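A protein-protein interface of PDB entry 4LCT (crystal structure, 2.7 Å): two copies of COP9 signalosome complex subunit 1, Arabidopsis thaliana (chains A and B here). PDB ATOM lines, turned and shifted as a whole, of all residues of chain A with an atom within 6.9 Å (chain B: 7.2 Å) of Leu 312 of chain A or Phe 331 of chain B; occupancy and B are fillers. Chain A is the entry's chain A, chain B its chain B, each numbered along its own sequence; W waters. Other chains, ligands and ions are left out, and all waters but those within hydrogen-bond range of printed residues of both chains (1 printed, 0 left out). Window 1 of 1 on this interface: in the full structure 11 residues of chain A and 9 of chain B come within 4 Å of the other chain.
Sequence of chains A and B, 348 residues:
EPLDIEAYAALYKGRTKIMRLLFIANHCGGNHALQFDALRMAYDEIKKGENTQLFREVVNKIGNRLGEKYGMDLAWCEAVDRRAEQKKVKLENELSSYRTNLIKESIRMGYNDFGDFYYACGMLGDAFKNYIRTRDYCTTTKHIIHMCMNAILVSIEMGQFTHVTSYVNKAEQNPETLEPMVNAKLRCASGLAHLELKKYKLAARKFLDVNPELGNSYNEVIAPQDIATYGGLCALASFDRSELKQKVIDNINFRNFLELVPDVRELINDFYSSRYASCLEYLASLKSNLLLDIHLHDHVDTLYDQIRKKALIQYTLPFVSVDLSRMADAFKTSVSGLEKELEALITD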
ATOM      1  N   PHE A 271     -35.291  10.628  22.385  1.00  0.00           N
ATOM      2  CA  PHE A 271     -35.595  11.363  23.614  1.00  0.00           C
ATOM      3  C   PHE A 271     -36.220  10.461  24.658  1.00  0.00           C
ATOM      4  O   PHE A 271     -35.902  10.543  25.846  1.00  0.00           O
ATOM      5  CB  PHE A 271     -36.548  12.522  23.320  1.00  0.00           C
ATOM      6  CG  PHE A 271     -36.942  13.325  24.538  1.00  0.00           C
ATOM      7  CD1 PHE A 271     -36.223  14.459  24.904  1.00  0.00           C
ATOM      8  CD2 PHE A 271     -38.057  12.976  25.288  1.00  0.00           C
ATOM      9  CE1 PHE A 271     -36.602  15.220  26.012  1.00  0.00           C
ATOM     10  CE2 PHE A 271     -38.431  13.721  26.395  1.00  0.00           C
ATOM     11  CZ  PHE A 271     -37.703  14.846  26.757  1.00  0.00           C
ATOM     12  N   TYR A 276     -29.526  11.060  24.777  1.00  0.00           N
ATOM     13  CA  TYR A 276     -29.686  12.490  24.671  1.00  0.00           C
ATOM     14  C   TYR A 276     -28.916  13.113  23.530  1.00  0.00           C
ATOM     15  O   TYR A 276     -29.469  13.924  22.789  1.00  0.00           O
ATOM     16  CB  TYR A 276     -29.288  13.119  25.997  1.00  0.00           C
ATOM     17  CG  TYR A 276     -30.132  12.607  27.134  1.00  0.00           C
ATOM     18  CD1 TYR A 276     -31.478  12.858  27.171  1.00  0.00           C
ATOM     19  CD2 TYR A 276     -29.579  11.884  28.159  1.00  0.00           C
ATOM     20  CE1 TYR A 276     -32.254  12.406  28.188  1.00  0.00           C
ATOM     21  CE2 TYR A 276     -30.340  11.422  29.179  1.00  0.00           C
ATOM     22  CZ  TYR A 276     -31.694  11.688  29.198  1.00  0.00           C
ATOM     23  OH  TYR A 276     -32.519  11.244  30.226  1.00  0.00           O
ATOM     24  N   ALA A 277     -27.643  12.747  23.410  1.00  0.00           N
ATOM     25  CA  ALA A 277     -26.760  13.318  22.394  1.00  0.00           C
ATOM     26  C   ALA A 277     -27.328  13.062  21.002  1.00  0.00           C
ATOM     27  O   ALA A 277     -27.268  13.922  20.123  1.00  0.00           O
ATOM     28  CB  ALA A 277     -25.362  12.741  22.514  1.00  0.00           C
ATOM     29  N   LEU A 280     -30.174  15.525  20.491  1.00  0.00           N
ATOM     30  CA  LEU A 280     -29.763  16.901  20.257  1.00  0.00           C
ATOM     31  C   LEU A 280     -29.074  17.025  18.897  1.00  0.00           C
ATOM     32  O   LEU A 280     -29.088  18.092  18.293  1.00  0.00           O
ATOM     33  CB  LEU A 280     -28.886  17.434  21.397  1.00  0.00           C
ATOM     34  CG  LEU A 280     -29.467  17.412  22.811  1.00  0.00           C
ATOM     35  CD1 LEU A 280     -28.336  17.452  23.818  1.00  0.00           C
ATOM     36  CD2 LEU A 280     -30.458  18.552  23.057  1.00  0.00           C
ATOM     37  N   ILE A 307     -37.528  21.515  25.217  1.00  0.00           N
ATOM     38  CA  ILE A 307     -37.146  20.123  25.048  1.00  0.00           C
ATOM     39  C   ILE A 307     -35.856  19.876  25.834  1.00  0.00           C
ATOM     40  O   ILE A 307     -35.820  19.028  26.739  1.00  0.00           O
ATOM     41  CB  ILE A 307     -36.998  19.756  23.569  1.00  0.00           C
ATOM     42  CG1 ILE A 307     -38.371  19.817  22.890  1.00  0.00           C
ATOM     43  CG2 ILE A 307     -36.384  18.379  23.416  1.00  0.00           C
ATOM     44  CD1 ILE A 307     -38.359  19.425  21.427  1.00  0.00           C
ATOM     45  N   ARG A 308     -34.835  20.681  25.536  1.00  0.00           N
ATOM     46  CA  ARG A 308     -33.534  20.549  26.173  1.00  0.00           C
ATOM     47  C   ARG A 308     -33.676  20.508  27.698  1.00  0.00           C
ATOM     48  O   ARG A 308     -33.058  19.669  28.357  1.00  0.00           O
ATOM     49  CB  ARG A 308     -32.613  21.696  25.749  1.00  0.00           C
ATOM     50  CG  ARG A 308     -31.199  21.589  26.303  1.00  0.00           C
ATOM     51  CD  ARG A 308     -30.267  22.642  25.710  1.00  0.00           C
ATOM     52  NE  ARG A 308     -28.889  22.429  26.140  1.00  0.00           N
ATOM     53  CZ  ARG A 308     -28.000  21.679  25.492  1.00  0.00           C
ATOM     54  NH1 ARG A 308     -28.339  21.070  24.360  1.00  0.00           N
ATOM     55  NH2 ARG A 308     -26.770  21.538  25.975  1.00  0.00           N
ATOM     56  N   LYS A 309     -34.518  21.386  28.250  1.00  0.00           N
ATOM     57  CA  LYS A 309     -34.642  21.486  29.699  1.00  0.00           C
ATOM     58  C   LYS A 309     -35.099  20.118  30.202  1.00  0.00           C
ATOM     59  O   LYS A 309     -34.453  19.507  31.059  1.00  0.00           O
ATOM     60  CB  LYS A 309     -35.655  22.572  30.073  1.00  0.00           C
ATOM     61  CG  LYS A 309     -35.256  23.511  31.212  1.00  0.00           C
ATOM     62  CD  LYS A 309     -36.159  24.759  31.213  1.00  0.00           C
ATOM     63  CE  LYS A 309     -36.067  25.544  32.520  1.00  0.00           C
ATOM     64  NZ  LYS A 309     -34.669  26.014  32.792  1.00  0.00           N
ATOM     65  N   LYS A 310     -36.197  19.623  29.632  1.00  0.00           N
ATOM     66  CA  LYS A 310     -36.722  18.319  30.010  1.00  0.00           C
ATOM     67  C   LYS A 310     -35.618  17.260  29.960  1.00  0.00           C
ATOM     68  O   LYS A 310     -35.480  16.443  30.874  1.00  0.00           O
ATOM     69  CB  LYS A 310     -37.909  17.923  29.122  1.00  0.00           C
ATOM     70  CG  LYS A 310     -39.250  18.500  29.586  1.00  0.00           C
ATOM     71  CD  LYS A 310     -40.398  18.037  28.681  1.00  0.00           C
ATOM     72  CE  LYS A 310     -41.752  18.340  29.297  1.00  0.00           C
ATOM     73  NZ  LYS A 310     -41.841  19.769  29.768  1.00  0.00           N
ATOM     74  N   ALA A 311     -34.797  17.301  28.921  1.00  0.00           N
ATOM     75  CA  ALA A 311     -33.808  16.255  28.761  1.00  0.00           C
ATOM     76  C   ALA A 311     -32.886  16.292  29.970  1.00  0.00           C
ATOM     77  O   ALA A 311     -32.618  15.255  30.584  1.00  0.00           O
ATOM     78  CB  ALA A 311     -33.027  16.440  27.470  1.00  0.00           C
ATOM     79  N   LEU A 312     -32.437  17.498  30.323  1.00  0.00           N
ATOM     80  CA  LEU A 312     -31.530  17.676  31.450  1.00  0.00           C
ATOM     81  C   LEU A 312     -32.162  17.049  32.685  1.00  0.00           C
ATOM     82  O   LEU A 312     -31.508  16.303  33.420  1.00  0.00           O
ATOM     83  CB  LEU A 312     -31.233  19.156  31.730  1.00  0.00           C
ATOM     84  CG  LEU A 312     -30.270  19.990  30.882  1.00  0.00           C
ATOM     85  CD1 LEU A 312     -29.900  21.253  31.637  1.00  0.00           C
ATOM     86  CD2 LEU A 312     -29.016  19.217  30.525  1.00  0.00           C
ATOM     87  N   ILE A 313     -33.443  17.327  32.913  1.00  0.00           N
ATOM     88  CA  ILE A 313     -34.037  16.830  34.140  1.00  0.00           C
ATOM     89  C   ILE A 313     -34.066  15.310  34.086  1.00  0.00           C
ATOM     90  O   ILE A 313     -33.758  14.649  35.077  1.00  0.00           O
ATOM     91  CB  ILE A 313     -35.423  17.417  34.398  1.00  0.00           C
ATOM     92  CG1 ILE A 313     -35.314  18.937  34.500  1.00  0.00           C
ATOM     93  CG2 ILE A 313     -36.013  16.851  35.682  1.00  0.00           C
ATOM     94  CD1 ILE A 313     -36.560  19.658  34.014  1.00  0.00           C
ATOM     95  N   GLN A 314     -34.391  14.759  32.917  1.00  0.00           N
ATOM     96  CA  GLN A 314     -34.440  13.309  32.791  1.00  0.00           C
ATOM     97  C   GLN A 314     -33.087  12.748  33.206  1.00  0.00           C
ATOM     98  O   GLN A 314     -33.011  11.726  33.890  1.00  0.00           O
ATOM     99  CB  GLN A 314     -34.780  12.864  31.364  1.00  0.00           C
ATOM    100  CG  GLN A 314     -35.508  11.538  31.296  1.00  0.00           C
ATOM    101  CD  GLN A 314     -36.677  11.496  32.275  1.00  0.00           C
ATOM    102  OE1 GLN A 314     -37.267  12.529  32.615  1.00  0.00           O
ATOM    103  NE2 GLN A 314     -37.014  10.298  32.738  1.00  0.00           N
ATOM    104  N   TYR A 315     -32.027  13.446  32.817  1.00  0.00           N
ATOM    105  CA  TYR A 315     -30.694  12.935  33.038  1.00  0.00           C
ATOM    106  C   TYR A 315     -30.411  12.783  34.535  1.00  0.00           C
ATOM    107  O   TYR A 315     -29.715  11.848  34.948  1.00  0.00           O
ATOM    108  CB  TYR A 315     -29.658  13.828  32.368  1.00  0.00           C
ATOM    109  CG  TYR A 315     -28.260  13.300  32.467  1.00  0.00           C
ATOM    110  CD1 TYR A 315     -27.663  12.693  31.386  1.00  0.00           C
ATOM    111  CD2 TYR A 315     -27.531  13.408  33.655  1.00  0.00           C
ATOM    112  CE1 TYR A 315     -26.358  12.209  31.463  1.00  0.00           C
ATOM    113  CE2 TYR A 315     -26.232  12.927  33.749  1.00  0.00           C
ATOM    114  CZ  TYR A 315     -25.649  12.329  32.648  1.00  0.00           C
ATOM    115  OH  TYR A 315     -24.358  11.849  32.726  1.00  0.00           O
ATOM    116  N   THR A 316     -31.001  13.661  35.340  1.00  0.00           N
ATOM    117  CA  THR A 316     -30.693  13.694  36.757  1.00  0.00           C
ATOM    118  C   THR A 316     -31.469  12.670  37.598  1.00  0.00           C
ATOM    119  O   THR A 316     -31.240  12.549  38.805  1.00  0.00           O
ATOM    120  CB  THR A 316     -30.894  15.098  37.347  1.00  0.00           C
ATOM    121  OG1 THR A 316     -32.295  15.389  37.454  1.00  0.00           O
ATOM    122  CG2 THR A 316     -30.195  16.149  36.492  1.00  0.00           C
ATOM    123  N   LEU A 317     -32.385  11.943  36.964  1.00  0.00           N
ATOM    124  CA  LEU A 317     -33.027  10.797  37.597  1.00  0.00           C
ATOM    125  C   LEU A 317     -31.976   9.716  37.873  1.00  0.00           C
ATOM    126  O   LEU A 317     -31.156   9.405  37.003  1.00  0.00           O
ATOM    127  CB  LEU A 317     -34.091  10.224  36.667  1.00  0.00           C
ATOM    128  CG  LEU A 317     -35.447   9.882  37.270  1.00  0.00           C
ATOM    129  CD1 LEU A 317     -35.437  10.184  38.752  1.00  0.00           C
ATOM    130  CD2 LEU A 317     -36.548  10.667  36.581  1.00  0.00           C
ATOM    131  N   SER B 325     -18.412  15.846  33.439  1.00  0.00           N
ATOM    132  CA  SER B 325     -17.957  15.772  32.062  1.00  0.00           C
ATOM    133  C   SER B 325     -18.804  14.752  31.325  1.00  0.00           C
ATOM    134  O   SER B 325     -19.024  14.904  30.113  1.00  0.00           O
ATOM    135  CB  SER B 325     -16.459  15.464  31.969  1.00  0.00           C
ATOM    136  OG  SER B 325     -16.238  14.075  31.815  1.00  0.00           O
ATOM    137  N   ARG B 326     -19.290  13.731  32.046  1.00  0.00           N
ATOM    138  CA  ARG B 326     -20.145  12.723  31.415  1.00  0.00           C
ATOM    139  C   ARG B 326     -21.411  13.403  30.872  1.00  0.00           C
ATOM    140  O   ARG B 326     -21.807  13.221  29.710  1.00  0.00           O
ATOM    141  CB  ARG B 326     -20.511  11.567  32.363  1.00  0.00           C
ATOM    142  CG  ARG B 326     -21.542  10.600  31.711  1.00  0.00           C
ATOM    143  CD  ARG B 326     -21.923   9.347  32.510  1.00  0.00           C
ATOM    144  NE  ARG B 326     -20.761   8.511  32.805  1.00  0.00           N
ATOM    145  CZ  ARG B 326     -20.226   7.607  31.979  1.00  0.00           C
ATOM    146  NH1 ARG B 326     -20.740   7.390  30.774  1.00  0.00           N
ATOM    147  NH2 ARG B 326     -19.163   6.916  32.363  1.00  0.00           N
ATOM    148  N   MET B 327     -22.027  14.206  31.724  1.00  0.00           N
ATOM    149  CA  MET B 327     -23.224  14.926  31.345  1.00  0.00           C
ATOM    150  C   MET B 327     -22.926  15.918  30.206  1.00  0.00           C
ATOM    151  O   MET B 327     -23.619  15.932  29.187  1.00  0.00           O
ATOM    152  CB  MET B 327     -23.829  15.622  32.565  1.00  0.00           C
ATOM    153  CG  MET B 327     -25.226  16.048  32.352  1.00  0.00           C
ATOM    154  SD  MET B 327     -25.931  16.570  33.914  1.00  0.00           S
ATOM    155  CE  MET B 327     -27.621  16.834  33.394  1.00  0.00           C
ATOM    156  N   ALA B 328     -21.869  16.711  30.365  1.00  0.00           N
ATOM    157  CA  ALA B 328     -21.448  17.642  29.328  1.00  0.00           C
ATOM    158  C   ALA B 328     -21.414  16.927  27.988  1.00  0.00           C
ATOM    159  O   ALA B 328     -21.903  17.445  26.981  1.00  0.00           O
ATOM    160  CB  ALA B 328     -20.074  18.228  29.651  1.00  0.00           C
ATOM    161  N   ASP B 329     -20.839  15.733  27.971  1.00  0.00           N
ATOM    162  CA  ASP B 329     -20.739  15.007  26.712  1.00  0.00           C
ATOM    163  C   ASP B 329     -22.114  14.543  26.240  1.00  0.00           C
ATOM    164  O   ASP B 329     -22.415  14.590  25.047  1.00  0.00           O
ATOM    165  CB  ASP B 329     -19.726  13.860  26.793  1.00  0.00           C
ATOM    166  CG  ASP B 329     -18.298  14.355  27.078  1.00  0.00           C
ATOM    167  OD1 ASP B 329     -18.031  15.574  26.904  1.00  0.00           O
ATOM    168  OD2 ASP B 329     -17.444  13.520  27.480  1.00  0.00           O
ATOM    169  N   ALA B 330     -22.965  14.129  27.171  1.00  0.00           N
ATOM    170  CA  ALA B 330     -24.344  13.774  26.813  1.00  0.00           C
ATOM    171  C   ALA B 330     -25.125  14.967  26.235  1.00  0.00           C
ATOM    172  O   ALA B 330     -26.069  14.796  25.466  1.00  0.00           O
ATOM    173  CB  ALA B 330     -25.076  13.211  28.007  1.00  0.00           C
ATOM    174  N   PHE B 331     -24.782  16.165  26.683  1.00  0.00           N
ATOM    175  CA  PHE B 331     -25.471  17.358  26.233  1.00  0.00           C
ATOM    176  C   PHE B 331     -24.735  18.205  25.179  1.00  0.00           C
ATOM    177  O   PHE B 331     -25.171  19.325  24.836  1.00  0.00           O
ATOM    178  CB  PHE B 331     -26.057  18.122  27.417  1.00  0.00           C
ATOM    179  CG  PHE B 331     -27.285  17.463  27.969  1.00  0.00           C
ATOM    180  CD1 PHE B 331     -28.553  17.841  27.528  1.00  0.00           C
ATOM    181  CD2 PHE B 331     -27.175  16.405  28.862  1.00  0.00           C
ATOM    182  CE1 PHE B 331     -29.704  17.204  28.016  1.00  0.00           C
ATOM    183  CE2 PHE B 331     -28.297  15.766  29.353  1.00  0.00           C
ATOM    184  CZ  PHE B 331     -29.574  16.167  28.932  1.00  0.00           C
ATOM    185  N   LYS B 332     -23.607  17.674  24.705  1.00  0.00           N
ATOM    186  CA  LYS B 332     -22.807  18.335  23.680  1.00  0.00           C
ATOM    187  C   LYS B 332     -22.481  19.769  24.081  1.00  0.00           C
ATOM    188  O   LYS B 332     -22.695  20.701  23.304  1.00  0.00           O
ATOM    189  CB  LYS B 332     -23.541  18.319  22.334  1.00  0.00           C
ATOM    190  CG  LYS B 332     -24.329  17.032  22.093  1.00  0.00           C
ATOM    191  CD  LYS B 332     -24.021  16.451  20.703  1.00  0.00           C
ATOM    192  CE  LYS B 332     -22.542  16.099  20.563  1.00  0.00           C
ATOM    193  NZ  LYS B 332     -22.059  16.247  19.155  1.00  0.00           N
ATOM    194  N   THR B 333     -21.985  19.940  25.304  1.00  0.00           N
ATOM    195  CA  THR B 333     -21.475  21.240  25.753  1.00  0.00           C
ATOM    196  C   THR B 333     -20.160  21.061  26.462  1.00  0.00           C
ATOM    197  O   THR B 333     -19.696  19.934  26.675  1.00  0.00           O
ATOM    198  CB  THR B 333     -22.384  21.937  26.793  1.00  0.00           C
ATOM    199  OG1 THR B 333     -23.240  20.972  27.416  1.00  0.00           O
ATOM    200  CG2 THR B 333     -23.201  23.044  26.179  1.00  0.00           C
ATOM    201  N   SER B 334     -19.602  22.196  26.866  1.00  0.00           N
ATOM    202  CA  SER B 334     -18.481  22.227  27.777  1.00  0.00           C
ATOM    203  C   SER B 334     -19.015  22.065  29.210  1.00  0.00           C
ATOM    204  O   SER B 334     -20.232  22.060  29.426  1.00  0.00           O
ATOM    205  CB  SER B 334     -17.741  23.558  27.607  1.00  0.00           C
ATOM    206  OG  SER B 334     -18.444  24.623  28.230  1.00  0.00           O
ATOM    207  N   LEU B 338     -22.722  23.584  30.699  1.00  0.00           N
ATOM    208  CA  LEU B 338     -23.578  22.720  31.504  1.00  0.00           C
ATOM    209  C   LEU B 338     -23.823  23.331  32.886  1.00  0.00           C
ATOM    210  O   LEU B 338     -24.955  23.370  33.348  1.00  0.00           O
ATOM    211  CB  LEU B 338     -22.976  21.319  31.628  1.00  0.00           C
ATOM    212  CG  LEU B 338     -23.712  20.294  32.501  1.00  0.00           C
ATOM    213  CD1 LEU B 338     -25.148  20.097  32.038  1.00  0.00           C
ATOM    214  CD2 LEU B 338     -22.959  18.964  32.505  1.00  0.00           C
ATOM    215  N   LYS B 340     -23.879  26.379  33.684  1.00  0.00           N
ATOM    216  CA  LYS B 340     -24.909  27.416  33.533  1.00  0.00           C
ATOM    217  C   LYS B 340     -26.331  26.843  33.500  1.00  0.00           C
ATOM    218  O   LYS B 340     -27.241  27.288  34.236  1.00  0.00           O
ATOM    219  CB  LYS B 340     -24.665  28.248  32.285  1.00  0.00           C
ATOM    220  CG  LYS B 340     -23.536  29.248  32.386  1.00  0.00           C
ATOM    221  CD  LYS B 340     -23.481  30.034  31.090  1.00  0.00           C
ATOM    222  CE  LYS B 340     -22.162  30.735  30.848  1.00  0.00           C
ATOM    223  NZ  LYS B 340     -22.198  31.414  29.513  1.00  0.00           N
ATOM    224  N   GLU B 341     -26.517  25.864  32.625  1.00  0.00           N
ATOM    225  CA  GLU B 341     -27.808  25.193  32.542  1.00  0.00           C
ATOM    226  C   GLU B 341     -28.275  24.684  33.919  1.00  0.00           C
ATOM    227  O   GLU B 341     -29.397  24.967  34.370  1.00  0.00           O
ATOM    228  CB  GLU B 341     -27.734  24.032  31.545  1.00  0.00           C
ATOM    229  CG  GLU B 341     -27.106  24.422  30.214  1.00  0.00           C
ATOM    230  CD  GLU B 341     -27.664  23.611  29.054  1.00  0.00           C
ATOM    231  OE1 GLU B 341     -26.870  22.890  28.404  1.00  0.00           O
ATOM    232  OE2 GLU B 341     -28.893  23.704  28.785  1.00  0.00           O
ATOM    233  N   LEU B 342     -27.400  23.938  34.592  1.00  0.00           N
ATOM    234  CA  LEU B 342     -27.720  23.346  35.887  1.00  0.00           C
ATOM    235  C   LEU B 342     -28.083  24.412  36.931  1.00  0.00           C
ATOM    236  O   LEU B 342     -29.071  24.278  37.659  1.00  0.00           O
ATOM    237  CB  LEU B 342     -26.600  22.408  36.332  1.00  0.00           C
ATOM    238  CG  LEU B 342     -26.581  21.162  35.425  1.00  0.00           C
ATOM    239  CD1 LEU B 342     -25.420  20.209  35.716  1.00  0.00           C
ATOM    240  CD2 LEU B 342     -27.909  20.420  35.531  1.00  0.00           C
ATOM    241  N   ALA B 344     -29.377  27.217  36.351  1.00  0.00           N
ATOM    242  CA  ALA B 344     -30.706  27.681  35.966  1.00  0.00           C
ATOM    243  C   ALA B 344     -31.760  26.769  36.565  1.00  0.00           C
ATOM    244  O   ALA B 344     -32.673  27.224  37.274  1.00  0.00           O
ATOM    245  CB  ALA B 344     -30.848  27.739  34.462  1.00  0.00           C
ATOM    246  N   LEU B 345     -31.612  25.477  36.292  1.00  0.00           N
ATOM    247  CA  LEU B 345     -32.499  24.467  36.866  1.00  0.00           C
ATOM    248  C   LEU B 345     -32.631  24.561  38.389  1.00  0.00           C
ATOM    249  O   LEU B 345     -33.729  24.558  38.936  1.00  0.00           O
ATOM    250  CB  LEU B 345     -31.989  23.077  36.510  1.00  0.00           C
ATOM    251  CG  LEU B 345     -32.935  22.181  35.727  1.00  0.00           C
ATOM    252  CD1 LEU B 345     -33.367  22.867  34.446  1.00  0.00           C
ATOM    253  CD2 LEU B 345     -32.255  20.852  35.421  1.00  0.00           C
HETATM  254  O   HOH W   1     -31.404  25.326  32.252  1.00  0.00           O
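OE1 of Glu 341 of chain B is in salt-bridge range of NH2 of Arg 308 of chain A, at 2.8 Å.
The backbone NH (N) of Ala 277 of chain A lies within hydrogen-bond range of the backbone carbonyl oxygen (O) of Ala 330 of chain B (3.3 Å).
The guanidinium group of Arg 308 of chain A lies within hydrogen-bond range of the backbone carbonyl oxygen of Phe 331 of chain B.
The backbone NH (N) of Met 327 of chain B is in hydrogen-bond range of the side-chain hydroxyl (OH) of Tyr 315 of chain A (3.5 Å).
No position is printed for both chains.
Of the 17 pairs that touch across the chains among the printed residues, none has its exchanged pair printed and touching as well.
Phe 331 of chain B touches just these residues of chain A: Leu 280 (3.7 Å), Arg 308 (3.0 Å), Ala 311 (3.5 Å), Leu 312 (3.3 Å) and Tyr 315 (3.7 Å).
Ala 311 of chain A touches one residue of chain B.
Of the printed residues of chain A, Glu 341 of chain B touches Arg 308 (2.8 Å) and Leu 312 (3.5 Å).
Of the printed residues of chain A, Thr 333 of chain B touches Arg 308.
Of the printed residues of chain A, Arg 326 of chain B touches Tyr 315.
Ala 344 of chain B touches none of the printed residues of chain A.
Asp 329 of chain B touches none of the printed residues of chain A.
The nearest printed residue of chain B that does not touch Leu 280 of chain A is Lys 332 of chain B (4.4 Å).
Among the printed residues, pairs that only touch across the chains: Tyr 276 of chain A with Ala 330 of chain B (3.7 Å), Leu 280 of chain A with Ala 330 of chain B (3.9 Å), Leu 280 of chain A with Phe 331 of chain B (3.7 Å), Arg 308 of chain A with Thr 333 of chain B (3.9 Å), Lys 309 of chain A with Leu 345 of chain B (3.8 Å), Ala 311 of chain A with Phe 331 of chain B (3.5 Å), Leu 312 of chain A with Met 327 of chain B (3.9 Å), Leu 312 of chain A with Phe 331 of chain B (3.3 Å), Leu 312 of chain A with Glu 341 of chain B (3.5 Å), Ile 313 of chain A with Leu 345 of chain B (3.7 Å), Tyr 315 of chain A with Arg 326 of chain B (3.2 Å), Tyr 315 of chain A with Ala 330 of chain B (3.8 Å) and Tyr 315 of chain A with Phe 331 of chain B (3.7 Å).
Printed residues of chain B that touch a printed residue of chain A: Arg 326, Met 327, Ala 330, Phe 331, Thr 333, Glu 341 and Leu 345.
Hydrophobic or aromatic side chains of chain B within 4 Å of the printed part of chain A: Met 327, Ala 330, Phe 331 and Leu 345.
Hydrophobic or aromatic side chains of chain A within 4 Å of the printed part of chain B: Tyr 276, Ala 277, Leu 280, Ala 311, Leu 312, Ile 313 and Tyr 315.
Among the printed residues, 17 pairs touch across the chains.
Among the printed residues, Asp or Glu carboxylates within 4 Å of a Lys or Arg side-chain nitrogen of the other chain: Arg 308 of chain A with Glu 341 of chain B (2.8 Å).
Water W1 lies within hydrogen-bond range of O of Glu 341 of chain B (2.9 Å) and NZ of Lys 309 of chain A (3.4 Å).
The backbone NH (N) of Thr 333 of chain B lies within hydrogen-bond range of the backbone carbonyl oxygen (O) of Ala 328 of chain B, at 3.0 Å.
N of Tyr 315 of chain A is in hydrogen-bond range of OH of Tyr 276 of chain A (3.4 Å).
The backbone carbonyl oxygen of Ile 313 of chain A sits at hydrogen-bond distance from the side-chain hydroxyl of Thr 316 of chain A (2.9 Å).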
